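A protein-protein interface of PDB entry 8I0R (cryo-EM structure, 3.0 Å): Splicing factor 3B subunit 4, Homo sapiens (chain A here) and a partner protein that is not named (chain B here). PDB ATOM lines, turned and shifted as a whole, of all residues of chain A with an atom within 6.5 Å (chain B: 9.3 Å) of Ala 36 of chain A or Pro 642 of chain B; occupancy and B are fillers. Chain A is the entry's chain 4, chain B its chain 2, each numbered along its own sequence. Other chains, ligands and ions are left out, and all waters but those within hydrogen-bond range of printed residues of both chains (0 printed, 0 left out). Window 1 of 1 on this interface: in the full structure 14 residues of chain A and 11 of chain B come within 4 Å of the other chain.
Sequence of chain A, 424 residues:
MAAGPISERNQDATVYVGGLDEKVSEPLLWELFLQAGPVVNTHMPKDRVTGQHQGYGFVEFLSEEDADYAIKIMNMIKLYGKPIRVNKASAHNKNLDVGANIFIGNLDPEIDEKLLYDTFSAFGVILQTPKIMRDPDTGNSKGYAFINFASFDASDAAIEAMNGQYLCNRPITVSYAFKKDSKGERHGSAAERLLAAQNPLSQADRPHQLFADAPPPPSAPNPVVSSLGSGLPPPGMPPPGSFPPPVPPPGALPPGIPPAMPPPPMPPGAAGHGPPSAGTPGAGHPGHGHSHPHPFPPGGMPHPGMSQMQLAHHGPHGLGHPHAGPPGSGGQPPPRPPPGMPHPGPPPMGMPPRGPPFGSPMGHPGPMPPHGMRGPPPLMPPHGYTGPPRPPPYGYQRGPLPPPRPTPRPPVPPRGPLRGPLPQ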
ATOM      1  N   GLU A  31      -4.800   4.034  17.243  1.00  0.00           N
ATOM      2  CA  GLU A  31      -4.970   5.378  16.704  1.00  0.00           C
ATOM      3  C   GLU A  31      -3.804   5.742  15.799  1.00  0.00           C
ATOM      4  O   GLU A  31      -3.940   6.564  14.887  1.00  0.00           O
ATOM      5  CB  GLU A  31      -5.109   6.389  17.842  1.00  0.00           C
ATOM      6  N   LEU A  32      -2.639   5.145  16.051  1.00  0.00           N
ATOM      7  CA  LEU A  32      -1.531   5.282  15.116  1.00  0.00           C
ATOM      8  C   LEU A  32      -1.719   4.378  13.909  1.00  0.00           C
ATOM      9  O   LEU A  32      -1.403   4.776  12.783  1.00  0.00           O
ATOM     10  CB  LEU A  32      -0.205   4.973  15.809  1.00  0.00           C
ATOM     11  N   PHE A  33      -2.220   3.159  14.118  1.00  0.00           N
ATOM     12  CA  PHE A  33      -2.521   2.287  12.990  1.00  0.00           C
ATOM     13  C   PHE A  33      -3.616   2.857  12.095  1.00  0.00           C
ATOM     14  O   PHE A  33      -3.570   2.654  10.879  1.00  0.00           O
ATOM     15  CB  PHE A  33      -2.920   0.900  13.492  1.00  0.00           C
ATOM     16  N   LEU A  34      -4.585   3.577  12.666  1.00  0.00           N
ATOM     17  CA  LEU A  34      -5.675   4.146  11.879  1.00  0.00           C
ATOM     18  C   LEU A  34      -5.215   5.379  11.118  1.00  0.00           C
ATOM     19  O   LEU A  34      -5.640   5.617   9.982  1.00  0.00           O
ATOM     20  CB  LEU A  34      -6.853   4.485  12.791  1.00  0.00           C
ATOM     21  N   GLN A  35      -4.361   6.192  11.746  1.00  0.00           N
ATOM     22  CA  GLN A  35      -3.775   7.357  11.093  1.00  0.00           C
ATOM     23  C   GLN A  35      -2.858   6.976   9.938  1.00  0.00           C
ATOM     24  O   GLN A  35      -2.539   7.833   9.110  1.00  0.00           O
ATOM     25  CB  GLN A  35      -3.007   8.192  12.117  1.00  0.00           C
ATOM     26  N   ALA A  36      -2.440   5.714   9.861  1.00  0.00           N
ATOM     27  CA  ALA A  36      -1.631   5.238   8.747  1.00  0.00           C
ATOM     28  C   ALA A  36      -2.432   4.420   7.739  1.00  0.00           C
ATOM     29  O   ALA A  36      -2.160   4.497   6.537  1.00  0.00           O
ATOM     30  CB  ALA A  36      -0.455   4.407   9.272  1.00  0.00           C
ATOM     31  N   GLY A  37      -3.435   3.668   8.190  1.00  0.00           N
ATOM     32  CA  GLY A  37      -4.103   2.716   7.337  1.00  0.00           C
ATOM     33  C   GLY A  37      -5.301   2.063   7.992  1.00  0.00           C
ATOM     34  O   GLY A  37      -5.634   2.337   9.148  1.00  0.00           O
ATOM     35  N   PRO A  38      -5.972   1.170   7.263  1.00  0.00           N
ATOM     36  CA  PRO A  38      -7.291   0.662   7.708  1.00  0.00           C
ATOM     37  C   PRO A  38      -7.193  -0.255   8.924  1.00  0.00           C
ATOM     38  O   PRO A  38      -7.204  -1.486   8.841  1.00  0.00           O
ATOM     39  CB  PRO A  38      -7.802  -0.080   6.470  1.00  0.00           C
ATOM     40  N   GLU A  65       0.362  -3.834   1.800  1.00  0.00           N
ATOM     41  CA  GLU A  65       1.236  -2.682   1.605  1.00  0.00           C
ATOM     42  C   GLU A  65       1.022  -1.636   2.692  1.00  0.00           C
ATOM     43  O   GLU A  65       1.962  -0.916   3.057  1.00  0.00           O
ATOM     44  CB  GLU A  65       1.011  -2.079   0.220  1.00  0.00           C
ATOM     45  N   ASP A  66      -0.199  -1.542   3.224  1.00  0.00           N
ATOM     46  CA  ASP A  66      -0.422  -0.720   4.408  1.00  0.00           C
ATOM     47  C   ASP A  66       0.444  -1.186   5.564  1.00  0.00           C
ATOM     48  O   ASP A  66       1.121  -0.373   6.197  1.00  0.00           O
ATOM     49  CB  ASP A  66      -1.889  -0.762   4.819  1.00  0.00           C
ATOM     50  N   TYR A  69       4.291  -0.281   4.725  1.00  0.00           N
ATOM     51  CA  TYR A  69       4.717   1.093   4.968  1.00  0.00           C
ATOM     52  C   TYR A  69       4.466   1.496   6.418  1.00  0.00           C
ATOM     53  O   TYR A  69       5.159   2.368   6.953  1.00  0.00           O
ATOM     54  CB  TYR A  69       4.018   2.037   3.998  1.00  0.00           C
ATOM     55  N   ALA A  70       3.515   0.836   7.087  1.00  0.00           N
ATOM     56  CA  ALA A  70       3.335   1.020   8.522  1.00  0.00           C
ATOM     57  C   ALA A  70       4.558   0.566   9.300  1.00  0.00           C
ATOM     58  O   ALA A  70       5.003   1.269  10.210  1.00  0.00           O
ATOM     59  CB  ALA A  70       2.100   0.256   8.994  1.00  0.00           C
ATOM     60  N   ILE A  73       7.301   3.000   8.799  1.00  0.00           N
ATOM     61  CA  ILE A  73       7.136   4.296   9.445  1.00  0.00           C
ATOM     62  C   ILE A  73       7.237   4.161  10.956  1.00  0.00           C
ATOM     63  O   ILE A  73       7.641   5.102  11.648  1.00  0.00           O
ATOM     64  CB  ILE A  73       5.799   4.947   9.044  1.00  0.00           C
ATOM     65  N   GLU B 603     -12.621   7.126  12.834  1.00  0.00           N
ATOM     66  CA  GLU B 603     -11.688   8.246  12.744  1.00  0.00           C
ATOM     67  C   GLU B 603     -10.468   7.816  11.933  1.00  0.00           C
ATOM     68  O   GLU B 603      -9.402   7.499  12.467  1.00  0.00           O
ATOM     69  CB  GLU B 603     -11.286   8.729  14.131  1.00  0.00           C
ATOM     70  CG  GLU B 603     -12.380   9.457  14.895  1.00  0.00           C
ATOM     71  CD  GLU B 603     -13.134   8.540  15.836  1.00  0.00           C
ATOM     72  OE1 GLU B 603     -12.476   7.739  16.528  1.00  0.00           O
ATOM     73  OE2 GLU B 603     -14.376   8.641  15.907  1.00  0.00           O
ATOM     74  N   LYS B 604     -10.631   7.822  10.609  1.00  0.00           N
ATOM     75  CA  LYS B 604      -9.602   7.418   9.651  1.00  0.00           C
ATOM     76  C   LYS B 604      -8.509   8.499   9.400  1.00  0.00           C
ATOM     77  O   LYS B 604      -7.594   8.216   8.609  1.00  0.00           O
ATOM     78  CB  LYS B 604     -10.274   7.034   8.332  1.00  0.00           C
ATOM     79  CG  LYS B 604     -11.017   5.708   8.386  1.00  0.00           C
ATOM     80  CD  LYS B 604     -11.577   5.314   7.028  1.00  0.00           C
ATOM     81  CE  LYS B 604     -12.682   6.261   6.594  1.00  0.00           C
ATOM     82  NZ  LYS B 604     -13.059   6.086   5.171  1.00  0.00           N
ATOM     83  N   LYS B 605      -8.537   9.678  10.029  1.00  0.00           N
ATOM     84  CA  LYS B 605      -7.702  10.790   9.593  1.00  0.00           C
ATOM     85  C   LYS B 605      -6.435  10.946  10.429  1.00  0.00           C
ATOM     86  O   LYS B 605      -6.508  11.063  11.658  1.00  0.00           O
ATOM     87  CB  LYS B 605      -8.507  12.088   9.627  1.00  0.00           C
ATOM     88  N   PRO B 606      -5.258  10.963   9.792  1.00  0.00           N
ATOM     89  CA  PRO B 606      -4.018  11.182  10.552  1.00  0.00           C
ATOM     90  C   PRO B 606      -3.899  12.577  11.135  1.00  0.00           C
ATOM     91  O   PRO B 606      -3.235  12.750  12.166  1.00  0.00           O
ATOM     92  CB  PRO B 606      -2.921  10.918   9.514  1.00  0.00           C
ATOM     93  N   GLY B 607      -4.505  13.582  10.499  1.00  0.00           N
ATOM     94  CA  GLY B 607      -4.437  14.930  11.035  1.00  0.00           C
ATOM     95  C   GLY B 607      -4.995  15.019  12.440  1.00  0.00           C
ATOM     96  O   GLY B 607      -4.536  15.828  13.251  1.00  0.00           O
ATOM     97  N   ASP B 608      -5.986  14.190  12.751  1.00  0.00           N
ATOM     98  CA  ASP B 608      -6.515  14.162  14.105  1.00  0.00           C
ATOM     99  C   ASP B 608      -5.461  13.627  15.064  1.00  0.00           C
ATOM    100  O   ASP B 608      -5.184  12.423  15.106  1.00  0.00           O
ATOM    101  CB  ASP B 608      -7.773  13.297  14.165  1.00  0.00           C
ATOM    102  N   TRP B 632       5.898   9.801  12.903  1.00  0.00           N
ATOM    103  CA  TRP B 632       5.602   9.160  11.627  1.00  0.00           C
ATOM    104  C   TRP B 632       6.052   9.981  10.422  1.00  0.00           C
ATOM    105  O   TRP B 632       6.200   9.423   9.330  1.00  0.00           O
ATOM    106  CB  TRP B 632       4.104   8.870  11.520  1.00  0.00           C
ATOM    107  N   ALA B 635       9.774   8.900   8.535  1.00  0.00           N
ATOM    108  CA  ALA B 635       9.646   7.818   7.572  1.00  0.00           C
ATOM    109  C   ALA B 635       8.537   8.066   6.560  1.00  0.00           C
ATOM    110  O   ALA B 635       8.532   7.431   5.501  1.00  0.00           O
ATOM    111  CB  ALA B 635       9.411   6.493   8.292  1.00  0.00           C
ATOM    112  N   MET B 636       7.623   9.000   6.836  1.00  0.00           N
ATOM    113  CA  MET B 636       6.693   9.445   5.805  1.00  0.00           C
ATOM    114  C   MET B 636       7.439  10.098   4.651  1.00  0.00           C
ATOM    115  O   MET B 636       7.278   9.706   3.491  1.00  0.00           O
ATOM    116  CB  MET B 636       5.673  10.410   6.407  1.00  0.00           C
ATOM    117  N   GLN B 637       8.274  11.092   4.954  1.00  0.00           N
ATOM    118  CA  GLN B 637       9.136  11.685   3.937  1.00  0.00           C
ATOM    119  C   GLN B 637      10.110  10.681   3.337  1.00  0.00           C
ATOM    120  O   GLN B 637      10.523  10.855   2.184  1.00  0.00           O
ATOM    121  CB  GLN B 637       9.919  12.859   4.525  1.00  0.00           C
ATOM    122  N   TYR B 639       9.683   7.079   2.876  1.00  0.00           N
ATOM    123  CA  TYR B 639       9.107   6.047   2.021  1.00  0.00           C
ATOM    124  C   TYR B 639       7.625   6.259   1.737  1.00  0.00           C
ATOM    125  O   TYR B 639       6.889   5.278   1.591  1.00  0.00           O
ATOM    126  CB  TYR B 639       9.324   4.665   2.640  1.00  0.00           C
ATOM    127  N   GLY B 640       7.169   7.506   1.655  1.00  0.00           N
ATOM    128  CA  GLY B 640       5.786   7.791   1.370  1.00  0.00           C
ATOM    129  C   GLY B 640       4.921   7.670   2.607  1.00  0.00           C
ATOM    130  O   GLY B 640       5.380   7.276   3.683  1.00  0.00           O
ATOM    131  N   PRO B 641       3.645   8.016   2.480  1.00  0.00           N
ATOM    132  CA  PRO B 641       2.685   7.683   3.530  1.00  0.00           C
ATOM    133  C   PRO B 641       2.421   6.189   3.536  1.00  0.00           C
ATOM    134  O   PRO B 641       2.819   5.481   2.600  1.00  0.00           O
ATOM    135  CB  PRO B 641       1.430   8.476   3.132  1.00  0.00           C
ATOM    136  N   PRO B 642       1.781   5.667   4.575  1.00  0.00           N
ATOM    137  CA  PRO B 642       1.480   4.237   4.604  1.00  0.00           C
ATOM    138  C   PRO B 642       0.585   3.858   3.442  1.00  0.00           C
ATOM    139  O   PRO B 642      -0.300   4.632   3.050  1.00  0.00           O
ATOM    140  CB  PRO B 642       0.776   4.046   5.952  1.00  0.00           C
ATOM    141  N   PRO B 643       0.786   2.678   2.853  1.00  0.00           N
ATOM    142  CA  PRO B 643       0.166   2.409   1.549  1.00  0.00           C
ATOM    143  C   PRO B 643      -1.286   1.973   1.629  1.00  0.00           C
ATOM    144  O   PRO B 643      -1.816   1.474   0.628  1.00  0.00           O
ATOM    145  CB  PRO B 643       1.056   1.310   0.958  1.00  0.00           C
ATOM    146  N   SER B 644      -1.944   2.123   2.781  1.00  0.00           N
ATOM    147  CA  SER B 644      -3.396   2.244   2.767  1.00  0.00           C
ATOM    148  C   SER B 644      -3.829   3.689   2.635  1.00  0.00           C
ATOM    149  O   SER B 644      -4.947   3.949   2.180  1.00  0.00           O
ATOM    150  CB  SER B 644      -4.021   1.661   4.031  1.00  0.00           C
ATOM    151  N   TYR B 645      -2.959   4.624   3.005  1.00  0.00           N
ATOM    152  CA  TYR B 645      -3.256   6.052   2.979  1.00  0.00           C
ATOM    153  C   TYR B 645      -2.436   6.695   1.870  1.00  0.00           C
ATOM    154  O   TYR B 645      -1.515   7.481   2.126  1.00  0.00           O
ATOM    155  CB  TYR B 645      -2.962   6.697   4.334  1.00  0.00           C
ATOM    156  N   PRO B 646      -2.735   6.362   0.614  1.00  0.00           N
ATOM    157  CA  PRO B 646      -2.344   7.263  -0.475  1.00  0.00           C
ATOM    158  C   PRO B 646      -2.906   8.658  -0.292  1.00  0.00           C
ATOM    159  O   PRO B 646      -2.250   9.641  -0.656  1.00  0.00           O
ATOM    160  CB  PRO B 646      -2.922   6.578  -1.720  1.00  0.00           C
ATOM    161  N   ASN B 647      -4.110   8.765   0.279  1.00  0.00           N
ATOM    162  CA  ASN B 647      -4.836  10.022   0.395  1.00  0.00           C
ATOM    163  C   ASN B 647      -4.641  10.715   1.738  1.00  0.00           C
ATOM    164  O   ASN B 647      -5.446  11.589   2.076  1.00  0.00           O
ATOM    165  CB  ASN B 647      -6.325   9.786   0.146  1.00  0.00           C
ATOM    166  N   LEU B 648      -3.622  10.359   2.516  1.00  0.00           N
ATOM    167  CA  LEU B 648      -3.273  11.141   3.694  1.00  0.00           C
ATOM    168  C   LEU B 648      -2.161  12.122   3.334  1.00  0.00           C
ATOM    169  O   LEU B 648      -1.207  11.756   2.639  1.00  0.00           O
ATOM    170  CB  LEU B 648      -2.844  10.227   4.839  1.00  0.00           C
ATOM    171  N   LYS B 649      -2.280  13.363   3.800  1.00  0.00           N
ATOM    172  CA  LYS B 649      -1.255  14.382   3.602  1.00  0.00           C
ATOM    173  C   LYS B 649      -0.538  14.633   4.920  1.00  0.00           C
ATOM    174  O   LYS B 649      -1.183  14.796   5.961  1.00  0.00           O
ATOM    175  CB  LYS B 649      -1.862  15.682   3.074  1.00  0.00           C
ATOM    176  N   ILE B 650       0.786  14.687   4.870  1.00  0.00           N
ATOM    177  CA  ILE B 650       1.636  14.711   6.057  1.00  0.00           C
ATOM    178  C   ILE B 650       1.912  16.166   6.418  1.00  0.00           C
ATOM    179  O   ILE B 650       2.247  16.961   5.534  1.00  0.00           O
ATOM    180  CB  ILE B 650       2.949  13.943   5.833  1.00  0.00           C
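Of the printed residues of chain B, Gln 35 of chain A touches Pro 606 (3.1 Å). Ala 36 of chain A touches two residues of chain B. Of chain B, only Ser 644 (3.5 Å) comes within 4 Å of Gly 37 of chain A. Printed residues of chain A within 4 Å of Glu 603 of chain B: Leu 34. Lys 605 of chain B touches none of the printed residues of chain A. Of the printed residues of chain A, Ala 635 of chain B touches Ile 73 (3.4 Å). Pro 642 of chain B touches two residues of chain A. Of the printed residues of chain A, Tyr 645 of chain B touches Ala 36. Lys 649 of chain B touches none of the printed residues of chain A. The nearest printed residue of chain A that does not touch Pro 606 of chain B is Ala 36 of chain A (5.2 Å).
Among the printed residues, pairs that only touch across the chains: Leu 34 of chain A with Glu 603 of chain B (3.96 Å), Leu 34 of chain A with Lys 604 of chain B (3.5 Å), Gln 35 of chain A with Pro 606 of chain B (3.1 Å), Ala 36 of chain A with Pro 642 of chain B (3.0 Å), Ala 36 of chain A with Tyr 645 of chain B (3.2 Å), Gly 37 of chain A with Ser 644 of chain B (3.5 Å), Pro 38 of chain A with Ser 644 of chain B (3.8 Å), Glu 65 of chain A with Pro 643 of chain B (3.2 Å), Asp 66 of chain A with Pro 643 of chain B (3.9 Å), Asp 66 of chain A with Ser 644 of chain B (3.3 Å), Tyr 69 of chain A with Pro 641 of chain B (3.9 Å), Tyr 69 of chain A with Pro 642 of chain B (3.4 Å), Tyr 69 of chain A with Pro 643 of chain B (3.5 Å) and Ile 73 of chain A with Ala 635 of chain B (3.4 Å).
Of the 22 printed residues of chain B, 9 touch a printed residue of chain A. Hydrophobic or aromatic side chains of chain B within 4 Å of the printed part of chain A: Pro 606, Ala 635, Pro 642, Pro 643 and Tyr 645. Hydrophobic or aromatic side chains of chain A within 4 Å of the printed part of chain B: Leu 34, Ala 36 and Tyr 69. Among the printed residues, 14 pairs touch across the chains. Among the printed residues, no Asp or Glu carboxylate lies within 4 Å of a Lys or Arg side-chain nitrogen of the other chain.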
